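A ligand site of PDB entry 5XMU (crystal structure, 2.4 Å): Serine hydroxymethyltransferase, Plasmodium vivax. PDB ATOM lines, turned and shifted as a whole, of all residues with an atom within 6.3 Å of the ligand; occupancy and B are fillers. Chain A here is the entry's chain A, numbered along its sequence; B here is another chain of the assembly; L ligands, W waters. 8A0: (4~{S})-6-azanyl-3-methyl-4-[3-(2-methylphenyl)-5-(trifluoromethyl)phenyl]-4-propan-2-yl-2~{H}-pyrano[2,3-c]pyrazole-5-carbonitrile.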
ATOM      1  N   HIS A 123      -8.882  35.374  23.809  1.00  0.00           N
ATOM      2  CA  HIS A 123      -9.989  35.494  22.895  1.00  0.00           C
ATOM      3  C   HIS A 123     -10.357  34.101  22.377  1.00  0.00           C
ATOM      4  O   HIS A 123      -9.505  33.233  22.247  1.00  0.00           O
ATOM      5  CB  HIS A 123      -9.612  36.420  21.729  1.00  0.00           C
ATOM      6  CG  HIS A 123     -10.780  37.123  21.129  1.00  0.00           C
ATOM      7  ND1 HIS A 123     -11.696  36.482  20.316  1.00  0.00           N
ATOM      8  CD2 HIS A 123     -11.210  38.402  21.230  1.00  0.00           C
ATOM      9  CE1 HIS A 123     -12.627  37.335  19.944  1.00  0.00           C
ATOM     10  NE2 HIS A 123     -12.360  38.511  20.490  1.00  0.00           N
ATOM     11  N   LEU A 124     -11.627  33.894  22.088  1.00  0.00           N
ATOM     12  CA  LEU A 124     -12.107  32.621  21.552  1.00  0.00           C
ATOM     13  C   LEU A 124     -11.452  32.291  20.213  1.00  0.00           C
ATOM     14  O   LEU A 124     -10.896  31.205  20.048  1.00  0.00           O
ATOM     15  CB  LEU A 124     -13.617  32.667  21.420  1.00  0.00           C
ATOM     16  CG  LEU A 124     -14.372  31.401  21.000  1.00  0.00           C
ATOM     17  CD1 LEU A 124     -14.589  30.412  22.124  1.00  0.00           C
ATOM     18  CD2 LEU A 124     -15.723  31.843  20.496  1.00  0.00           C
ATOM     19  N   CYS A 125     -11.507  33.256  19.280  1.00  0.00           N
ATOM     20  CA  CYS A 125     -10.694  33.274  18.033  1.00  0.00           C
ATOM     21  C   CYS A 125      -9.236  32.856  18.199  1.00  0.00           C
ATOM     22  O   CYS A 125      -8.706  32.182  17.333  1.00  0.00           O
ATOM     23  CB  CYS A 125     -10.668  34.664  17.371  1.00  0.00           C
ATOM     24  SG  CYS A 125     -11.703  34.870  15.881  1.00  0.00           S
ATOM     25  N   SER A 126      -8.580  33.296  19.269  1.00  0.00           N
ATOM     26  CA  SER A 126      -7.145  33.022  19.470  1.00  0.00           C
ATOM     27  C   SER A 126      -6.833  31.736  20.214  1.00  0.00           C
ATOM     28  O   SER A 126      -5.668  31.357  20.319  1.00  0.00           O
ATOM     29  CB  SER A 126      -6.465  34.200  20.152  1.00  0.00           C
ATOM     30  OG  SER A 126      -6.409  35.292  19.251  1.00  0.00           O
ATOM     31  N   GLY A 127      -7.864  31.044  20.718  1.00  0.00           N
ATOM     32  CA  GLY A 127      -7.663  29.755  21.400  1.00  0.00           C
ATOM     33  C   GLY A 127      -8.308  29.608  22.753  1.00  0.00           C
ATOM     34  O   GLY A 127      -8.311  28.525  23.299  1.00  0.00           O
ATOM     35  N   GLY A 128      -8.862  30.680  23.301  1.00  0.00           N
ATOM     36  CA  GLY A 128      -9.457  30.663  24.620  1.00  0.00           C
ATOM     37  C   GLY A 128     -10.849  30.085  24.585  1.00  0.00           C
ATOM     38  O   GLY A 128     -11.442  29.943  23.515  1.00  0.00           O
ATOM     39  N   HIS A 129     -11.364  29.737  25.758  1.00  0.00           N
ATOM     40  CA  HIS A 129     -12.715  29.206  25.876  1.00  0.00           C
ATOM     41  C   HIS A 129     -13.770  30.280  25.987  1.00  0.00           C
ATOM     42  O   HIS A 129     -13.487  31.441  26.224  1.00  0.00           O
ATOM     43  CB  HIS A 129     -12.811  28.195  27.040  1.00  0.00           C
ATOM     44  CG  HIS A 129     -13.968  27.253  26.889  1.00  0.00           C
ATOM     45  ND1 HIS A 129     -15.053  27.267  27.743  1.00  0.00           N
ATOM     46  CD2 HIS A 129     -14.245  26.316  25.948  1.00  0.00           C
ATOM     47  CE1 HIS A 129     -15.946  26.392  27.325  1.00  0.00           C
ATOM     48  NE2 HIS A 129     -15.466  25.778  26.264  1.00  0.00           N
ATOM     49  N   LEU A 130     -15.012  29.871  25.765  1.00  0.00           N
ATOM     50  CA  LEU A 130     -16.169  30.747  25.935  1.00  0.00           C
ATOM     51  C   LEU A 130     -16.282  31.280  27.367  1.00  0.00           C
ATOM     52  O   LEU A 130     -16.668  32.437  27.560  1.00  0.00           O
ATOM     53  CB  LEU A 130     -17.447  29.974  25.601  1.00  0.00           C
ATOM     54  CG  LEU A 130     -17.572  29.515  24.157  1.00  0.00           C
ATOM     55  CD1 LEU A 130     -18.512  28.329  24.109  1.00  0.00           C
ATOM     56  CD2 LEU A 130     -18.039  30.653  23.243  1.00  0.00           C
ATOM     57  N   PHE A 134     -15.442  35.511  26.931  1.00  0.00           N
ATOM     58  CA  PHE A 134     -15.702  35.820  25.537  1.00  0.00           C
ATOM     59  C   PHE A 134     -16.961  36.618  25.321  1.00  0.00           C
ATOM     60  O   PHE A 134     -18.018  36.239  25.834  1.00  0.00           O
ATOM     61  CB  PHE A 134     -15.828  34.577  24.678  1.00  0.00           C
ATOM     62  CG  PHE A 134     -16.179  34.889  23.259  1.00  0.00           C
ATOM     63  CD1 PHE A 134     -15.257  35.515  22.425  1.00  0.00           C
ATOM     64  CD2 PHE A 134     -17.457  34.626  22.779  1.00  0.00           C
ATOM     65  CE1 PHE A 134     -15.596  35.831  21.123  1.00  0.00           C
ATOM     66  CE2 PHE A 134     -17.785  34.935  21.473  1.00  0.00           C
ATOM     67  CZ  PHE A 134     -16.860  35.551  20.642  1.00  0.00           C
ATOM     68  N   VAL A 141     -21.633  37.209  24.765  1.00  0.00           N
ATOM     69  CA  VAL A 141     -21.924  35.829  24.347  1.00  0.00           C
ATOM     70  C   VAL A 141     -21.886  34.822  25.507  1.00  0.00           C
ATOM     71  O   VAL A 141     -22.672  33.872  25.549  1.00  0.00           O
ATOM     72  CB  VAL A 141     -20.943  35.390  23.213  1.00  0.00           C
ATOM     73  CG1 VAL A 141     -21.129  33.929  22.839  1.00  0.00           C
ATOM     74  CG2 VAL A 141     -21.164  36.263  21.971  1.00  0.00           C
ATOM     75  N   THR A 183      -8.580  26.282  24.897  1.00  0.00           N
ATOM     76  CA  THR A 183      -9.415  25.278  24.216  1.00  0.00           C
ATOM     77  C   THR A 183      -8.716  24.787  22.950  1.00  0.00           C
ATOM     78  O   THR A 183      -8.678  23.574  22.699  1.00  0.00           O
ATOM     79  CB  THR A 183     -10.905  25.680  24.029  1.00  0.00           C
ATOM     80  OG1 THR A 183     -11.346  25.440  22.684  1.00  0.00           O
ATOM     81  CG2 THR A 183     -11.118  27.058  24.318  1.00  0.00           C
ATOM     82  N   SER A 184      -8.112  25.701  22.189  1.00  0.00           N
ATOM     83  CA  SER A 184      -7.403  25.286  20.986  1.00  0.00           C
ATOM     84  C   SER A 184      -6.076  25.981  20.818  1.00  0.00           C
ATOM     85  O   SER A 184      -5.895  26.796  19.945  1.00  0.00           O
ATOM     86  CB  SER A 184      -8.286  25.479  19.763  1.00  0.00           C
ATOM     87  OG  SER A 184      -8.512  26.848  19.519  1.00  0.00           O
ATOM     88  N   ASN A 354     -13.045  19.418  13.746  1.00  0.00           N
ATOM     89  CA  ASN A 354     -13.855  20.600  13.841  1.00  0.00           C
ATOM     90  C   ASN A 354     -13.145  21.773  13.240  1.00  0.00           C
ATOM     91  O   ASN A 354     -11.896  21.843  13.223  1.00  0.00           O
ATOM     92  CB  ASN A 354     -14.278  20.869  15.290  1.00  0.00           C
ATOM     93  CG  ASN A 354     -13.120  21.241  16.200  1.00  0.00           C
ATOM     94  OD1 ASN A 354     -12.524  20.372  16.842  1.00  0.00           O
ATOM     95  ND2 ASN A 354     -12.808  22.553  16.264  1.00  0.00           N
ATOM     96  N   LYS A 355     -13.961  22.683  12.720  1.00  0.00           N
ATOM     97  CA  LYS A 355     -13.521  23.950  12.179  1.00  0.00           C
ATOM     98  C   LYS A 355     -12.943  24.802  13.288  1.00  0.00           C
ATOM     99  O   LYS A 355     -13.422  24.764  14.419  1.00  0.00           O
ATOM    100  CB  LYS A 355     -14.661  24.702  11.482  1.00  0.00           C
ATOM    101  CG  LYS A 355     -16.048  24.483  12.055  1.00  0.00           C
ATOM    102  CD  LYS A 355     -16.998  25.628  11.771  1.00  0.00           C
ATOM    103  CE  LYS A 355     -18.439  25.137  11.872  1.00  0.00           C
ATOM    104  NZ  LYS A 355     -19.417  26.251  11.790  1.00  0.00           N
ATOM    105  N   ASN A 356     -11.926  25.588  12.943  1.00  0.00           N
ATOM    106  CA  ASN A 356     -11.225  26.377  13.940  1.00  0.00           C
ATOM    107  C   ASN A 356     -10.665  27.627  13.336  1.00  0.00           C
ATOM    108  O   ASN A 356     -10.145  27.616  12.213  1.00  0.00           O
ATOM    109  CB  ASN A 356     -10.090  25.557  14.595  1.00  0.00           C
ATOM    110  CG  ASN A 356      -9.785  26.019  16.012  1.00  0.00           C
ATOM    111  OD1 ASN A 356     -10.374  25.529  16.970  1.00  0.00           O
ATOM    112  ND2 ASN A 356      -8.911  26.994  16.141  1.00  0.00           N
ATOM    113  N   THR A 357     -10.717  28.683  14.113  1.00  0.00           N
ATOM    114  CA  THR A 357     -10.177  29.960  13.712  1.00  0.00           C
ATOM    115  C   THR A 357      -8.644  29.934  13.724  1.00  0.00           C
ATOM    116  O   THR A 357      -8.018  29.026  14.305  1.00  0.00           O
ATOM    117  CB  THR A 357     -10.675  31.054  14.662  1.00  0.00           C
ATOM    118  OG1 THR A 357     -10.328  30.694  15.997  1.00  0.00           O
ATOM    119  CG2 THR A 357     -12.197  31.193  14.602  1.00  0.00           C
ATOM    120  N   CYS A 364     -14.701  35.842  13.251  1.00  0.00           N
ATOM    121  CA  CYS A 364     -15.133  34.440  13.415  1.00  0.00           C
ATOM    122  C   CYS A 364     -16.111  33.932  12.330  1.00  0.00           C
ATOM    123  O   CYS A 364     -16.476  32.742  12.340  1.00  0.00           O
ATOM    124  CB  CYS A 364     -15.816  34.253  14.796  1.00  0.00           C
ATOM    125  SG  CYS A 364     -14.831  33.397  16.036  1.00  0.00           S
ATOM    126  N   VAL A 365     -16.528  34.815  11.424  1.00  0.00           N
ATOM    127  CA  VAL A 365     -17.558  34.528  10.412  1.00  0.00           C
ATOM    128  C   VAL A 365     -17.150  33.328   9.559  1.00  0.00           C
ATOM    129  O   VAL A 365     -17.991  32.472   9.258  1.00  0.00           O
ATOM    130  CB  VAL A 365     -17.899  35.775   9.528  1.00  0.00           C
ATOM    131  CG1 VAL A 365     -18.560  35.373   8.208  1.00  0.00           C
ATOM    132  CG2 VAL A 365     -18.818  36.747  10.277  1.00  0.00           C
ATOM    133  N   SER A 366     -15.871  33.267   9.189  1.00  0.00           N
ATOM    134  CA  SER A 366     -15.342  32.102   8.500  1.00  0.00           C
ATOM    135  C   SER A 366     -14.046  31.600   9.174  1.00  0.00           C
ATOM    136  O   SER A 366     -13.008  32.281   9.061  1.00  0.00           O
ATOM    137  CB  SER A 366     -15.103  32.452   7.028  1.00  0.00           C
ATOM    138  OG  SER A 366     -16.327  32.475   6.317  1.00  0.00           O
ATOM    139  N   PRO A 367     -14.112  30.439   9.879  1.00  0.00           N
ATOM    140  CA  PRO A 367     -12.848  29.885  10.409  1.00  0.00           C
ATOM    141  C   PRO A 367     -11.938  29.354   9.276  1.00  0.00           C
ATOM    142  O   PRO A 367     -12.379  28.551   8.440  1.00  0.00           O
ATOM    143  CB  PRO A 367     -13.314  28.740  11.305  1.00  0.00           C
ATOM    144  CG  PRO A 367     -14.592  28.299  10.700  1.00  0.00           C
ATOM    145  CD  PRO A 367     -15.249  29.572  10.247  1.00  0.00           C
ATOM    146  N   GLY A 369      -9.429  27.344   9.456  1.00  0.00           N
ATOM    147  CA  GLY A 369      -8.722  26.121   9.749  1.00  0.00           C
ATOM    148  C   GLY A 369      -9.567  25.051  10.347  1.00  0.00           C
ATOM    149  O   GLY A 369     -10.798  25.155  10.448  1.00  0.00           O
ATOM    150  N   ARG A 371      -9.077  21.980  13.623  1.00  0.00           N
ATOM    151  CA  ARG A 371      -8.314  21.501  14.729  1.00  0.00           C
ATOM    152  C   ARG A 371      -8.453  20.004  14.799  1.00  0.00           C
ATOM    153  O   ARG A 371      -9.538  19.476  14.614  1.00  0.00           O
ATOM    154  CB  ARG A 371      -8.818  22.155  16.004  1.00  0.00           C
ATOM    155  CG  ARG A 371      -8.068  21.747  17.266  1.00  0.00           C
ATOM    156  CD  ARG A 371      -8.837  22.222  18.486  1.00  0.00           C
ATOM    157  NE  ARG A 371     -10.078  21.476  18.638  1.00  0.00           N
ATOM    158  CZ  ARG A 371     -10.894  21.555  19.685  1.00  0.00           C
ATOM    159  NH1 ARG A 371     -10.631  22.343  20.741  1.00  0.00           N
ATOM    160  NH2 ARG A 371     -12.001  20.818  19.687  1.00  0.00           N
ATOM    161  N   GLU B  56     -21.902  20.658  20.942  1.00  0.00           N
ATOM    162  CA  GLU B  56     -22.329  22.022  21.264  1.00  0.00           C
ATOM    163  C   GLU B  56     -23.287  22.619  20.243  1.00  0.00           C
ATOM    164  O   GLU B  56     -23.145  22.388  19.070  1.00  0.00           O
ATOM    165  CB  GLU B  56     -21.107  22.934  21.377  1.00  0.00           C
ATOM    166  CG  GLU B  56     -20.464  22.894  22.759  1.00  0.00           C
ATOM    167  CD  GLU B  56     -19.020  23.331  22.775  1.00  0.00           C
ATOM    168  OE1 GLU B  56     -18.203  22.566  22.266  1.00  0.00           O
ATOM    169  OE2 GLU B  56     -18.692  24.406  23.271  1.00  0.00           O
ATOM    170  N   TYR B  63     -22.043  22.749  16.096  1.00  0.00           N
ATOM    171  CA  TYR B  63     -20.744  23.241  15.711  1.00  0.00           C
ATOM    172  C   TYR B  63     -20.036  22.147  14.957  1.00  0.00           C
ATOM    173  O   TYR B  63     -19.475  22.411  13.897  1.00  0.00           O
ATOM    174  CB  TYR B  63     -19.931  23.826  16.893  1.00  0.00           C
ATOM    175  CG  TYR B  63     -20.353  25.261  17.067  1.00  0.00           C
ATOM    176  CD1 TYR B  63     -21.496  25.599  17.778  1.00  0.00           C
ATOM    177  CD2 TYR B  63     -19.692  26.283  16.381  1.00  0.00           C
ATOM    178  CE1 TYR B  63     -21.929  26.907  17.864  1.00  0.00           C
ATOM    179  CE2 TYR B  63     -20.128  27.599  16.465  1.00  0.00           C
ATOM    180  CZ  TYR B  63     -21.243  27.901  17.203  1.00  0.00           C
ATOM    181  OH  TYR B  63     -21.672  29.215  17.310  1.00  0.00           O
ATOM    182  N   TYR B  64     -20.122  20.921  15.457  1.00  0.00           N
ATOM    183  CA  TYR B  64     -19.487  19.777  14.781  1.00  0.00           C
ATOM    184  C   TYR B  64     -20.463  18.910  14.024  1.00  0.00           C
ATOM    185  O   TYR B  64     -21.644  18.915  14.300  1.00  0.00           O
ATOM    186  CB  TYR B  64     -18.751  18.886  15.749  1.00  0.00           C
ATOM    187  CG  TYR B  64     -17.903  19.605  16.734  1.00  0.00           C
ATOM    188  CD1 TYR B  64     -17.565  20.954  16.580  1.00  0.00           C
ATOM    189  CD2 TYR B  64     -17.411  18.922  17.861  1.00  0.00           C
ATOM    190  CE1 TYR B  64     -16.777  21.590  17.506  1.00  0.00           C
ATOM    191  CE2 TYR B  64     -16.607  19.554  18.790  1.00  0.00           C
ATOM    192  CZ  TYR B  64     -16.290  20.880  18.625  1.00  0.00           C
ATOM    193  OH  TYR B  64     -15.493  21.492  19.572  1.00  0.00           O
ATOM    194  N   PHE B 266     -26.899  27.587  26.013  1.00  0.00           N
ATOM    195  CA  PHE B 266     -25.628  27.616  25.307  1.00  0.00           C
ATOM    196  C   PHE B 266     -25.703  28.719  24.265  1.00  0.00           C
ATOM    197  O   PHE B 266     -26.664  28.766  23.530  1.00  0.00           O
ATOM    198  CB  PHE B 266     -25.355  26.309  24.604  1.00  0.00           C
ATOM    199  CG  PHE B 266     -24.162  26.349  23.683  1.00  0.00           C
ATOM    200  CD1 PHE B 266     -24.306  26.713  22.331  1.00  0.00           C
ATOM    201  CD2 PHE B 266     -22.882  26.038  24.156  1.00  0.00           C
ATOM    202  CE1 PHE B 266     -23.206  26.739  21.484  1.00  0.00           C
ATOM    203  CE2 PHE B 266     -21.785  26.051  23.304  1.00  0.00           C
ATOM    204  CZ  PHE B 266     -21.950  26.390  21.971  1.00  0.00           C
ATOM    205  N   PRO B 267     -24.675  29.549  24.145  1.00  0.00           N
ATOM    206  CA  PRO B 267     -23.376  29.385  24.803  1.00  0.00           C
ATOM    207  C   PRO B 267     -23.185  30.263  26.042  1.00  0.00           C
ATOM    208  O   PRO B 267     -22.087  30.378  26.547  1.00  0.00           O
ATOM    209  CB  PRO B 267     -22.405  29.845  23.707  1.00  0.00           C
ATOM    210  CG  PRO B 267     -23.164  30.953  23.034  1.00  0.00           C
ATOM    211  CD  PRO B 267     -24.639  30.597  23.113  1.00  0.00           C
HETATM  212  C5  8A0 L   1     -15.261  26.450  20.574  1.00  0.00           C
HETATM  213  C6  8A0 L   1     -14.710  26.719  21.880  1.00  0.00           C
HETATM  214  C8  8A0 L   1     -12.671  28.121  18.520  1.00  0.00           C
HETATM  215  C2  8A0 L   1     -12.799  27.877  20.818  1.00  0.00           C
HETATM  216  N7  8A0 L   1     -11.698  28.586  20.997  1.00  0.00           N
HETATM  217  C12 8A0 L   1     -17.650  25.279  20.043  1.00  0.00           C
HETATM  218  C16 8A0 L   1     -15.293  27.686  16.984  1.00  0.00           C
HETATM  219  F48 8A0 L   1     -14.855  27.900  14.205  1.00  0.00           F
HETATM  220  C33 8A0 L   1     -15.941  28.518  14.657  1.00  0.00           C
HETATM  221  F46 8A0 L   1     -17.013  28.005  14.075  1.00  0.00           F
HETATM  222  F47 8A0 L   1     -15.880  29.767  14.237  1.00  0.00           F
HETATM  223  C17 8A0 L   1     -16.110  28.506  16.185  1.00  0.00           C
HETATM  224  C18 8A0 L   1     -17.102  29.273  16.771  1.00  0.00           C
HETATM  225  C19 8A0 L   1     -17.284  29.260  18.152  1.00  0.00           C
HETATM  226  C32 8A0 L   1     -18.363  30.120  18.714  1.00  0.00           C
HETATM  227  C43 8A0 L   1     -19.417  29.528  19.366  1.00  0.00           C
HETATM  228  C42 8A0 L   1     -20.448  30.302  19.910  1.00  0.00           C
HETATM  229  C41 8A0 L   1     -20.439  31.682  19.789  1.00  0.00           C
HETATM  230  C40 8A0 L   1     -19.390  32.289  19.118  1.00  0.00           C
HETATM  231  C39 8A0 L   1     -18.347  31.523  18.588  1.00  0.00           C
HETATM  232  C50 8A0 L   1     -17.215  32.191  17.867  1.00  0.00           C
HETATM  233  C20 8A0 L   1     -16.462  28.488  18.961  1.00  0.00           C
HETATM  234  C15 8A0 L   1     -15.459  27.669  18.411  1.00  0.00           C
HETATM  235  C4  8A0 L   1     -14.546  26.813  19.308  1.00  0.00           C
HETATM  236  C13 8A0 L   1     -14.070  25.505  18.648  1.00  0.00           C
HETATM  237  C34 8A0 L   1     -13.256  24.588  19.579  1.00  0.00           C
HETATM  238  C14 8A0 L   1     -15.188  24.694  17.966  1.00  0.00           C
HETATM  239  C3  8A0 L   1     -13.299  27.653  19.528  1.00  0.00           C
HETATM  240  N9  8A0 L   1     -12.096  28.546  17.583  1.00  0.00           N
HETATM  241  C10 8A0 L   1     -16.547  25.799  20.926  1.00  0.00           C
HETATM  242  N51 8A0 L   1     -16.598  25.780  22.270  1.00  0.00           N
HETATM  243  N11 8A0 L   1     -15.483  26.357  22.906  1.00  0.00           N
HETATM  244  O1  8A0 L   1     -13.494  27.323  21.964  1.00  0.00           O
HETATM  245  O   HOH W   1      -9.339  29.068  19.054  1.00  0.00           O
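The backbone carbonyl oxygen (O) of Lys 355 sits close to a fluorine (F48) of the ligand (3.5 Å).
Residues that only touch the ligand: Gly 127 (3.95 Å), Leu 130 (3.7 Å), Phe 134 (3.9 Å), Val 141 (3.9 Å), Ser 184 (3.9 Å), Asn 354 (3.6 Å), Asn 356 (3.5 Å), Cys 364 (3.2 Å), Pro 367 (3.4 Å), Arg 371 (3.6 Å), Tyr 63 of chain B (3.1 Å) and Tyr 64 of chain B (3.5 Å).
Hydrophobic or aromatic side chains that line the ligand: Leu 124, His 129, Leu 130, Phe 134, Val 141, Pro 367, Tyr 63 of chain B and Tyr 64 of chain B.
Of the 27 residues printed, 19 come within 4 Å of the ligand.
The nearest printed residue that does not touch the ligand is Pro 267 of chain B (4.2 Å).
A nitrogen (N51) of the ligand lies within hydrogen-bond range of the side-chain carboxylate of Glu 56 of chain B (2.7 Å).
The backbone carbonyl oxygen (O) of Gly 128 sits at hydrogen-bond distance from a nitrogen (N7) of the ligand (2.9 Å).
The backbone carbonyl oxygen (O) of Leu 124 lies within hydrogen-bond range of a nitrogen (N7) of the ligand (2.9 Å).
An oxygen (O1) of the ligand is in hydrogen-bond range of the side-chain hydroxyl (OG1) of Thr 183 (2.9 Å).
OG1 of Thr 357 lies within hydrogen-bond range of N9 of the ligand, at 3.2 Å.
NE2 of His 129 sits close to N11 of the ligand.
The backbone NH of Tyr 63 of chain B sits at hydrogen-bond distance from the backbone carbonyl oxygen of Glu 56 of chain B (3.2 Å).
N of Gly 128 sits at hydrogen-bond distance from O of His 123 (2.8 Å).
The backbone carbonyl oxygen of Thr 183 sits at hydrogen-bond distance from the guanidinium group of Arg 371, 3.0 Å away.
N of Thr 183 lies within hydrogen-bond range of O of Gly 127 (2.8 Å).
O of Cys 125 lies within hydrogen-bond range of OG1 of Thr 357.
The side-chain sulfur (SG) of Cys 364 lies within hydrogen-bond range of the side-chain sulfur (SG) of Cys 125, at 3.5 Å.
OG of Ser 184 sits at hydrogen-bond distance from ND2 of Asn 356 (3.4 Å).
The backbone NH (N) of Asn 356 is in hydrogen-bond range of the backbone carbonyl oxygen (O) of Gly 369 (2.8 Å).
Water W1 lies within hydrogen-bond range of OG of Ser 184, O of Leu 124, N of Gly 127 and N7 of the ligand.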
